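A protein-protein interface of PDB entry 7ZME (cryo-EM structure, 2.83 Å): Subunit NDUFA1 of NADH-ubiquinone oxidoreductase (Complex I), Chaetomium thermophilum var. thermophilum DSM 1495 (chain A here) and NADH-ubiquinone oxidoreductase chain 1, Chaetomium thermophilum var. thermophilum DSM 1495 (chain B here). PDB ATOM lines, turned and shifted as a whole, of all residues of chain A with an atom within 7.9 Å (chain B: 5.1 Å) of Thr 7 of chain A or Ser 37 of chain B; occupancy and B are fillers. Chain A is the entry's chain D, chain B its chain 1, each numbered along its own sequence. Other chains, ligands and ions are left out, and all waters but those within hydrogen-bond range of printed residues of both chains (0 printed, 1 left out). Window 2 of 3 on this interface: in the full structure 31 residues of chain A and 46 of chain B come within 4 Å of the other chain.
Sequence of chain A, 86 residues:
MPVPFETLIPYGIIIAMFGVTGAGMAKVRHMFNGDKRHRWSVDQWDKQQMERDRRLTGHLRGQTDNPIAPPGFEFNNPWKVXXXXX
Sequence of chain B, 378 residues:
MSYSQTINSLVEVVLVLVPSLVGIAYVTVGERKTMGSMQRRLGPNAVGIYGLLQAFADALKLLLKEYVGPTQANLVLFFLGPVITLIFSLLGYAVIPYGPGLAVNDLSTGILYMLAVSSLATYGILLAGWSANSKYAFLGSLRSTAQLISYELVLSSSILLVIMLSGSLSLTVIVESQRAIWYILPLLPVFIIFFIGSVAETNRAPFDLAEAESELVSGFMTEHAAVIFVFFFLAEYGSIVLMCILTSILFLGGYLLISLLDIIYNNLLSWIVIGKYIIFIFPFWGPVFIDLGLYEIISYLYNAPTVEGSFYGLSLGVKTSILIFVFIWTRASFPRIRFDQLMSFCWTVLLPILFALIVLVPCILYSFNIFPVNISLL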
ATOM      1  N   VAL A   3       7.304   1.217  34.700  1.00  0.00           N
ATOM      2  CA  VAL A   3       7.334   0.963  33.264  1.00  0.00           C
ATOM      3  C   VAL A   3       6.491  -0.276  32.980  1.00  0.00           C
ATOM      4  O   VAL A   3       6.793  -1.350  33.520  1.00  0.00           O
ATOM      5  CB  VAL A   3       8.765   0.779  32.750  1.00  0.00           C
ATOM      6  CG1 VAL A   3       8.746   0.330  31.296  1.00  0.00           C
ATOM      7  CG2 VAL A   3       9.551   2.069  32.903  1.00  0.00           C
ATOM      8  N   PRO A   4       5.443  -0.176  32.168  1.00  0.00           N
ATOM      9  CA  PRO A   4       4.694  -1.363  31.724  1.00  0.00           C
ATOM     10  C   PRO A   4       5.384  -2.030  30.536  1.00  0.00           C
ATOM     11  O   PRO A   4       5.093  -1.782  29.368  1.00  0.00           O
ATOM     12  CB  PRO A   4       3.326  -0.782  31.367  1.00  0.00           C
ATOM     13  CG  PRO A   4       3.587   0.641  31.003  1.00  0.00           C
ATOM     14  CD  PRO A   4       4.924   1.059  31.560  1.00  0.00           C
ATOM     15  N   PHE A   5       6.357  -2.887  30.846  1.00  0.00           N
ATOM     16  CA  PHE A   5       7.167  -3.498  29.799  1.00  0.00           C
ATOM     17  C   PHE A   5       6.337  -4.393  28.888  1.00  0.00           C
ATOM     18  O   PHE A   5       6.685  -4.578  27.717  1.00  0.00           O
ATOM     19  CB  PHE A   5       8.329  -4.275  30.425  1.00  0.00           C
ATOM     20  CG  PHE A   5       7.945  -5.621  30.981  1.00  0.00           C
ATOM     21  CD1 PHE A   5       7.509  -5.745  32.287  1.00  0.00           C
ATOM     22  CD2 PHE A   5       8.056  -6.765  30.206  1.00  0.00           C
ATOM     23  CE1 PHE A   5       7.169  -6.976  32.805  1.00  0.00           C
ATOM     24  CE2 PHE A   5       7.713  -7.997  30.717  1.00  0.00           C
ATOM     25  CZ  PHE A   5       7.270  -8.104  32.020  1.00  0.00           C
ATOM     26  N   GLU A   6       5.239  -4.951  29.397  1.00  0.00           N
ATOM     27  CA  GLU A   6       4.373  -5.767  28.556  1.00  0.00           C
ATOM     28  C   GLU A   6       3.613  -4.935  27.531  1.00  0.00           C
ATOM     29  O   GLU A   6       3.121  -5.489  26.544  1.00  0.00           O
ATOM     30  CB  GLU A   6       3.403  -6.561  29.429  1.00  0.00           C
ATOM     31  CG  GLU A   6       4.099  -7.507  30.391  1.00  0.00           C
ATOM     32  CD  GLU A   6       3.411  -7.591  31.738  1.00  0.00           C
ATOM     33  OE1 GLU A   6       2.192  -7.329  31.809  1.00  0.00           O
ATOM     34  OE2 GLU A   6       4.092  -7.916  32.731  1.00  0.00           O
ATOM     35  N   THR A   7       3.506  -3.622  27.743  1.00  0.00           N
ATOM     36  CA  THR A   7       2.920  -2.751  26.733  1.00  0.00           C
ATOM     37  C   THR A   7       3.877  -2.535  25.569  1.00  0.00           C
ATOM     38  O   THR A   7       3.441  -2.391  24.422  1.00  0.00           O
ATOM     39  CB  THR A   7       2.525  -1.413  27.366  1.00  0.00           C
ATOM     40  OG1 THR A   7       1.567  -1.640  28.405  1.00  0.00           O
ATOM     41  CG2 THR A   7       1.927  -0.471  26.337  1.00  0.00           C
ATOM     42  N   LEU A   8       5.178  -2.545  25.840  1.00  0.00           N
ATOM     43  CA  LEU A   8       6.205  -2.286  24.842  1.00  0.00           C
ATOM     44  C   LEU A   8       6.608  -3.526  24.054  1.00  0.00           C
ATOM     45  O   LEU A   8       7.478  -3.425  23.184  1.00  0.00           O
ATOM     46  CB  LEU A   8       7.441  -1.694  25.518  1.00  0.00           C
ATOM     47  CG  LEU A   8       7.214  -0.629  26.589  1.00  0.00           C
ATOM     48  CD1 LEU A   8       8.544  -0.102  27.079  1.00  0.00           C
ATOM     49  CD2 LEU A   8       6.365   0.503  26.050  1.00  0.00           C
ATOM     50  N   ILE A   9       6.018  -4.683  24.335  1.00  0.00           N
ATOM     51  CA  ILE A   9       6.401  -5.923  23.662  1.00  0.00           C
ATOM     52  C   ILE A   9       5.882  -5.924  22.225  1.00  0.00           C
ATOM     53  O   ILE A   9       6.645  -6.268  21.310  1.00  0.00           O
ATOM     54  CB  ILE A   9       5.917  -7.157  24.442  1.00  0.00           C
ATOM     55  CG1 ILE A   9       6.793  -7.395  25.668  1.00  0.00           C
ATOM     56  CG2 ILE A   9       5.935  -8.382  23.563  1.00  0.00           C
ATOM     57  CD1 ILE A   9       6.381  -8.595  26.482  1.00  0.00           C
ATOM     58  N   PRO A  10       4.617  -5.571  21.958  1.00  0.00           N
ATOM     59  CA  PRO A  10       4.191  -5.485  20.555  1.00  0.00           C
ATOM     60  C   PRO A  10       4.990  -4.488  19.741  1.00  0.00           C
ATOM     61  O   PRO A  10       5.174  -4.701  18.538  1.00  0.00           O
ATOM     62  CB  PRO A  10       2.718  -5.077  20.670  1.00  0.00           C
ATOM     63  CG  PRO A  10       2.294  -5.675  21.934  1.00  0.00           C
ATOM     64  CD  PRO A  10       3.452  -5.456  22.856  1.00  0.00           C
ATOM     65  N   TYR A  11       5.476  -3.410  20.359  1.00  0.00           N
ATOM     66  CA  TYR A  11       6.303  -2.458  19.629  1.00  0.00           C
ATOM     67  C   TYR A  11       7.666  -3.050  19.295  1.00  0.00           C
ATOM     68  O   TYR A  11       8.231  -2.760  18.237  1.00  0.00           O
ATOM     69  CB  TYR A  11       6.457  -1.172  20.435  1.00  0.00           C
ATOM     70  CG  TYR A  11       5.199  -0.340  20.487  1.00  0.00           C
ATOM     71  CD1 TYR A  11       4.766   0.369  19.377  1.00  0.00           C
ATOM     72  CD2 TYR A  11       4.447  -0.262  21.646  1.00  0.00           C
ATOM     73  CE1 TYR A  11       3.619   1.129  19.424  1.00  0.00           C
ATOM     74  CE2 TYR A  11       3.300   0.496  21.703  1.00  0.00           C
ATOM     75  CZ  TYR A  11       2.889   1.189  20.592  1.00  0.00           C
ATOM     76  OH  TYR A  11       1.744   1.945  20.650  1.00  0.00           O
ATOM     77  N   GLY A  12       8.214  -3.874  20.189  1.00  0.00           N
ATOM     78  CA  GLY A  12       9.463  -4.550  19.885  1.00  0.00           C
ATOM     79  C   GLY A  12       9.323  -5.548  18.752  1.00  0.00           C
ATOM     80  O   GLY A  12      10.249  -5.732  17.960  1.00  0.00           O
ATOM     81  N   GLY B  30      -0.740  -3.782  20.089  1.00  0.00           N
ATOM     82  CA  GLY B  30      -0.047  -2.695  20.752  1.00  0.00           C
ATOM     83  C   GLY B  30      -0.951  -1.517  21.050  1.00  0.00           C
ATOM     84  O   GLY B  30      -0.834  -0.889  22.103  1.00  0.00           O
ATOM     85  N   LYS B  33      -3.057  -2.479  24.064  1.00  0.00           N
ATOM     86  CA  LYS B  33      -2.234  -2.497  25.265  1.00  0.00           C
ATOM     87  C   LYS B  33      -1.693  -1.122  25.626  1.00  0.00           C
ATOM     88  O   LYS B  33      -1.418  -0.871  26.803  1.00  0.00           O
ATOM     89  CB  LYS B  33      -1.084  -3.487  25.099  1.00  0.00           C
ATOM     90  CG  LYS B  33      -1.543  -4.937  25.090  1.00  0.00           C
ATOM     91  CD  LYS B  33      -0.469  -5.878  25.599  1.00  0.00           C
ATOM     92  CE  LYS B  33      -0.412  -5.881  27.116  1.00  0.00           C
ATOM     93  NZ  LYS B  33      -1.643  -6.443  27.727  1.00  0.00           N
ATOM     94  N   THR B  34      -1.535  -0.230  24.649  1.00  0.00           N
ATOM     95  CA  THR B  34      -1.045   1.115  24.916  1.00  0.00           C
ATOM     96  C   THR B  34      -2.155   2.065  25.332  1.00  0.00           C
ATOM     97  O   THR B  34      -1.950   2.896  26.221  1.00  0.00           O
ATOM     98  CB  THR B  34      -0.326   1.667  23.686  1.00  0.00           C
ATOM     99  OG1 THR B  34       0.526   0.652  23.146  1.00  0.00           O
ATOM    100  CG2 THR B  34       0.506   2.883  24.053  1.00  0.00           C
ATOM    101  N   MET B  35      -3.330   1.965  24.710  1.00  0.00           N
ATOM    102  CA  MET B  35      -4.464   2.756  25.173  1.00  0.00           C
ATOM    103  C   MET B  35      -4.858   2.358  26.586  1.00  0.00           C
ATOM    104  O   MET B  35      -5.221   3.214  27.398  1.00  0.00           O
ATOM    105  CB  MET B  35      -5.649   2.599  24.222  1.00  0.00           C
ATOM    106  CG  MET B  35      -5.589   3.497  23.004  1.00  0.00           C
ATOM    107  SD  MET B  35      -7.141   3.530  22.096  1.00  0.00           S
ATOM    108  CE  MET B  35      -7.971   4.915  22.870  1.00  0.00           C
ATOM    109  N   GLY B  36      -4.785   1.063  26.898  1.00  0.00           N
ATOM    110  CA  GLY B  36      -5.100   0.616  28.243  1.00  0.00           C
ATOM    111  C   GLY B  36      -4.155   1.177  29.288  1.00  0.00           C
ATOM    112  O   GLY B  36      -4.582   1.583  30.369  1.00  0.00           O
ATOM    113  N   SER B  37      -2.857   1.206  28.981  1.00  0.00           N
ATOM    114  CA  SER B  37      -1.888   1.748  29.928  1.00  0.00           C
ATOM    115  C   SER B  37      -2.151   3.221  30.208  1.00  0.00           C
ATOM    116  O   SER B  37      -2.025   3.675  31.351  1.00  0.00           O
ATOM    117  CB  SER B  37      -0.469   1.543  29.402  1.00  0.00           C
ATOM    118  OG  SER B  37      -0.136   0.170  29.388  1.00  0.00           O
ATOM    119  N   MET B  38      -2.511   3.987  29.180  1.00  0.00           N
ATOM    120  CA  MET B  38      -2.897   5.374  29.399  1.00  0.00           C
ATOM    121  C   MET B  38      -4.259   5.489  30.066  1.00  0.00           C
ATOM    122  O   MET B  38      -4.590   6.551  30.598  1.00  0.00           O
ATOM    123  CB  MET B  38      -2.875   6.138  28.075  1.00  0.00           C
ATOM    124  CG  MET B  38      -1.630   5.869  27.253  1.00  0.00           C
ATOM    125  SD  MET B  38      -1.295   7.091  25.972  1.00  0.00           S
ATOM    126  CE  MET B  38      -2.177   6.374  24.597  1.00  0.00           C
ATOM    127  N   GLN B  39      -5.043   4.415  30.059  1.00  0.00           N
ATOM    128  CA  GLN B  39      -6.331   4.362  30.729  1.00  0.00           C
ATOM    129  C   GLN B  39      -6.264   3.607  32.049  1.00  0.00           C
ATOM    130  O   GLN B  39      -7.308   3.264  32.608  1.00  0.00           O
ATOM    131  CB  GLN B  39      -7.371   3.731  29.803  1.00  0.00           C
ATOM    132  CG  GLN B  39      -7.722   4.601  28.607  1.00  0.00           C
ATOM    133  CD  GLN B  39      -8.580   3.885  27.587  1.00  0.00           C
ATOM    134  OE1 GLN B  39      -8.897   2.711  27.740  1.00  0.00           O
ATOM    135  NE2 GLN B  39      -8.954   4.592  26.532  1.00  0.00           N
ATOM    136  N   ARG B  40      -5.053   3.355  32.554  1.00  0.00           N
ATOM    137  CA  ARG B  40      -4.810   2.606  33.790  1.00  0.00           C
ATOM    138  C   ARG B  40      -5.361   1.186  33.710  1.00  0.00           C
ATOM    139  O   ARG B  40      -5.824   0.628  34.705  1.00  0.00           O
ATOM    140  CB  ARG B  40      -5.366   3.339  35.015  1.00  0.00           C
ATOM    141  CG  ARG B  40      -5.067   4.832  35.045  1.00  0.00           C
ATOM    142  CD  ARG B  40      -3.618   5.128  35.383  1.00  0.00           C
ATOM    143  NE  ARG B  40      -3.209   4.569  36.668  1.00  0.00           N
ATOM    144  CZ  ARG B  40      -3.217   5.240  37.815  1.00  0.00           C
ATOM    145  NH1 ARG B  40      -3.618   6.502  37.846  1.00  0.00           N
ATOM    146  NH2 ARG B  40      -2.822   4.649  38.930  1.00  0.00           N
ATOM    147  N   ARG B  41      -5.308   0.598  32.522  1.00  0.00           N
ATOM    148  CA  ARG B  41      -5.699  -0.776  32.262  1.00  0.00           C
ATOM    149  C   ARG B  41      -4.463  -1.582  31.872  1.00  0.00           C
ATOM    150  O   ARG B  41      -3.328  -1.112  31.975  1.00  0.00           O
ATOM    151  CB  ARG B  41      -6.758  -0.833  31.160  1.00  0.00           C
ATOM    152  CG  ARG B  41      -8.000  -0.029  31.421  1.00  0.00           C
ATOM    153  CD  ARG B  41      -9.066  -0.358  30.397  1.00  0.00           C
ATOM    154  NE  ARG B  41      -8.851   0.300  29.110  1.00  0.00           N
ATOM    155  CZ  ARG B  41      -8.578  -0.338  27.976  1.00  0.00           C
ATOM    156  NH1 ARG B  41      -8.468  -1.657  27.963  1.00  0.00           N
ATOM    157  NH2 ARG B  41      -8.404   0.344  26.856  1.00  0.00           N
ATOM    158  N   LEU B  42      -4.680  -2.815  31.433  1.00  0.00           N
ATOM    159  CA  LEU B  42      -3.622  -3.641  30.867  1.00  0.00           C
ATOM    160  C   LEU B  42      -3.748  -3.840  29.366  1.00  0.00           C
ATOM    161  O   LEU B  42      -2.765  -3.672  28.643  1.00  0.00           O
ATOM    162  CB  LEU B  42      -3.596  -5.011  31.547  1.00  0.00           C
ATOM    163  CG  LEU B  42      -3.677  -5.014  33.070  1.00  0.00           C
ATOM    164  CD1 LEU B  42      -3.892  -6.419  33.581  1.00  0.00           C
ATOM    165  CD2 LEU B  42      -2.429  -4.409  33.686  1.00  0.00           C
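Of the printed residues of chain B, Glu 6 of chain A touches Lys 33 (3.6 Å). Of chain B, only Lys 33 (3.4 Å), Thr 34 (3.7 Å) and Ser 37 (2.7 Å) come within 4 Å of Thr 7 of chain A. Of the printed residues of chain B, Pro 10 of chain A touches Gly 30 (3.7 Å). Of the printed residues of chain A, Gly 30 of chain B touches Pro 10. Of the printed residues of chain A, Lys 33 of chain B touches Glu 6 and Thr 7. Printed residues of chain A within 4 Å of Thr 34 of chain B: Thr 7 (3.7 Å) and Tyr 11 (3.1 Å). The nearest residue of chain A that does not touch Ser 37 of chain B is Pro 4 of chain A (4.1 Å).
The side-chain hydroxyl (OG) of Ser 37 of chain B sits at hydrogen-bond distance from the side-chain hydroxyl (OG1) of Thr 7 of chain A (2.7 Å). The side-chain hydroxyl (OG1) of Thr 34 of chain B is in hydrogen-bond range of the side-chain hydroxyl (OH) of Tyr 11 of chain A, at 3.1 Å. OG1 of Thr 7 of chain A lies close to O of Lys 33 of chain B (3.5 Å).
Among the printed residues, merely in contact across the chains: Glu 6 of chain A with Lys 33 of chain B, Thr 7 of chain A with Thr 34 of chain B and Pro 10 of chain A with Gly 30 of chain B.
Hydrophobic or aromatic side chains of chain A within 4 Å of the printed part of chain B: Pro 10 and Tyr 11. Of the 11 printed residues of chain B, 4 touch a printed residue of chain A. Printed residues of chain B that touch a printed residue of chain A: Gly 30, Lys 33, Thr 34 and Ser 37. Among the printed residues, 6 pairs touch across the chains. Among the printed residues, no Asp or Glu carboxylate lies within 4 Å of a Lys or Arg side-chain nitrogen of the other chain.
The backbone carbonyl oxygen of Lys 33 of chain B sits at hydrogen-bond distance from the side-chain hydroxyl of Ser 37 of chain B (3.1 Å). The backbone carbonyl oxygen (O) of Leu 42 of chain B is in hydrogen-bond range of the side-chain amino group (NZ) of Lys 33 of chain B, at 3.1 Å.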
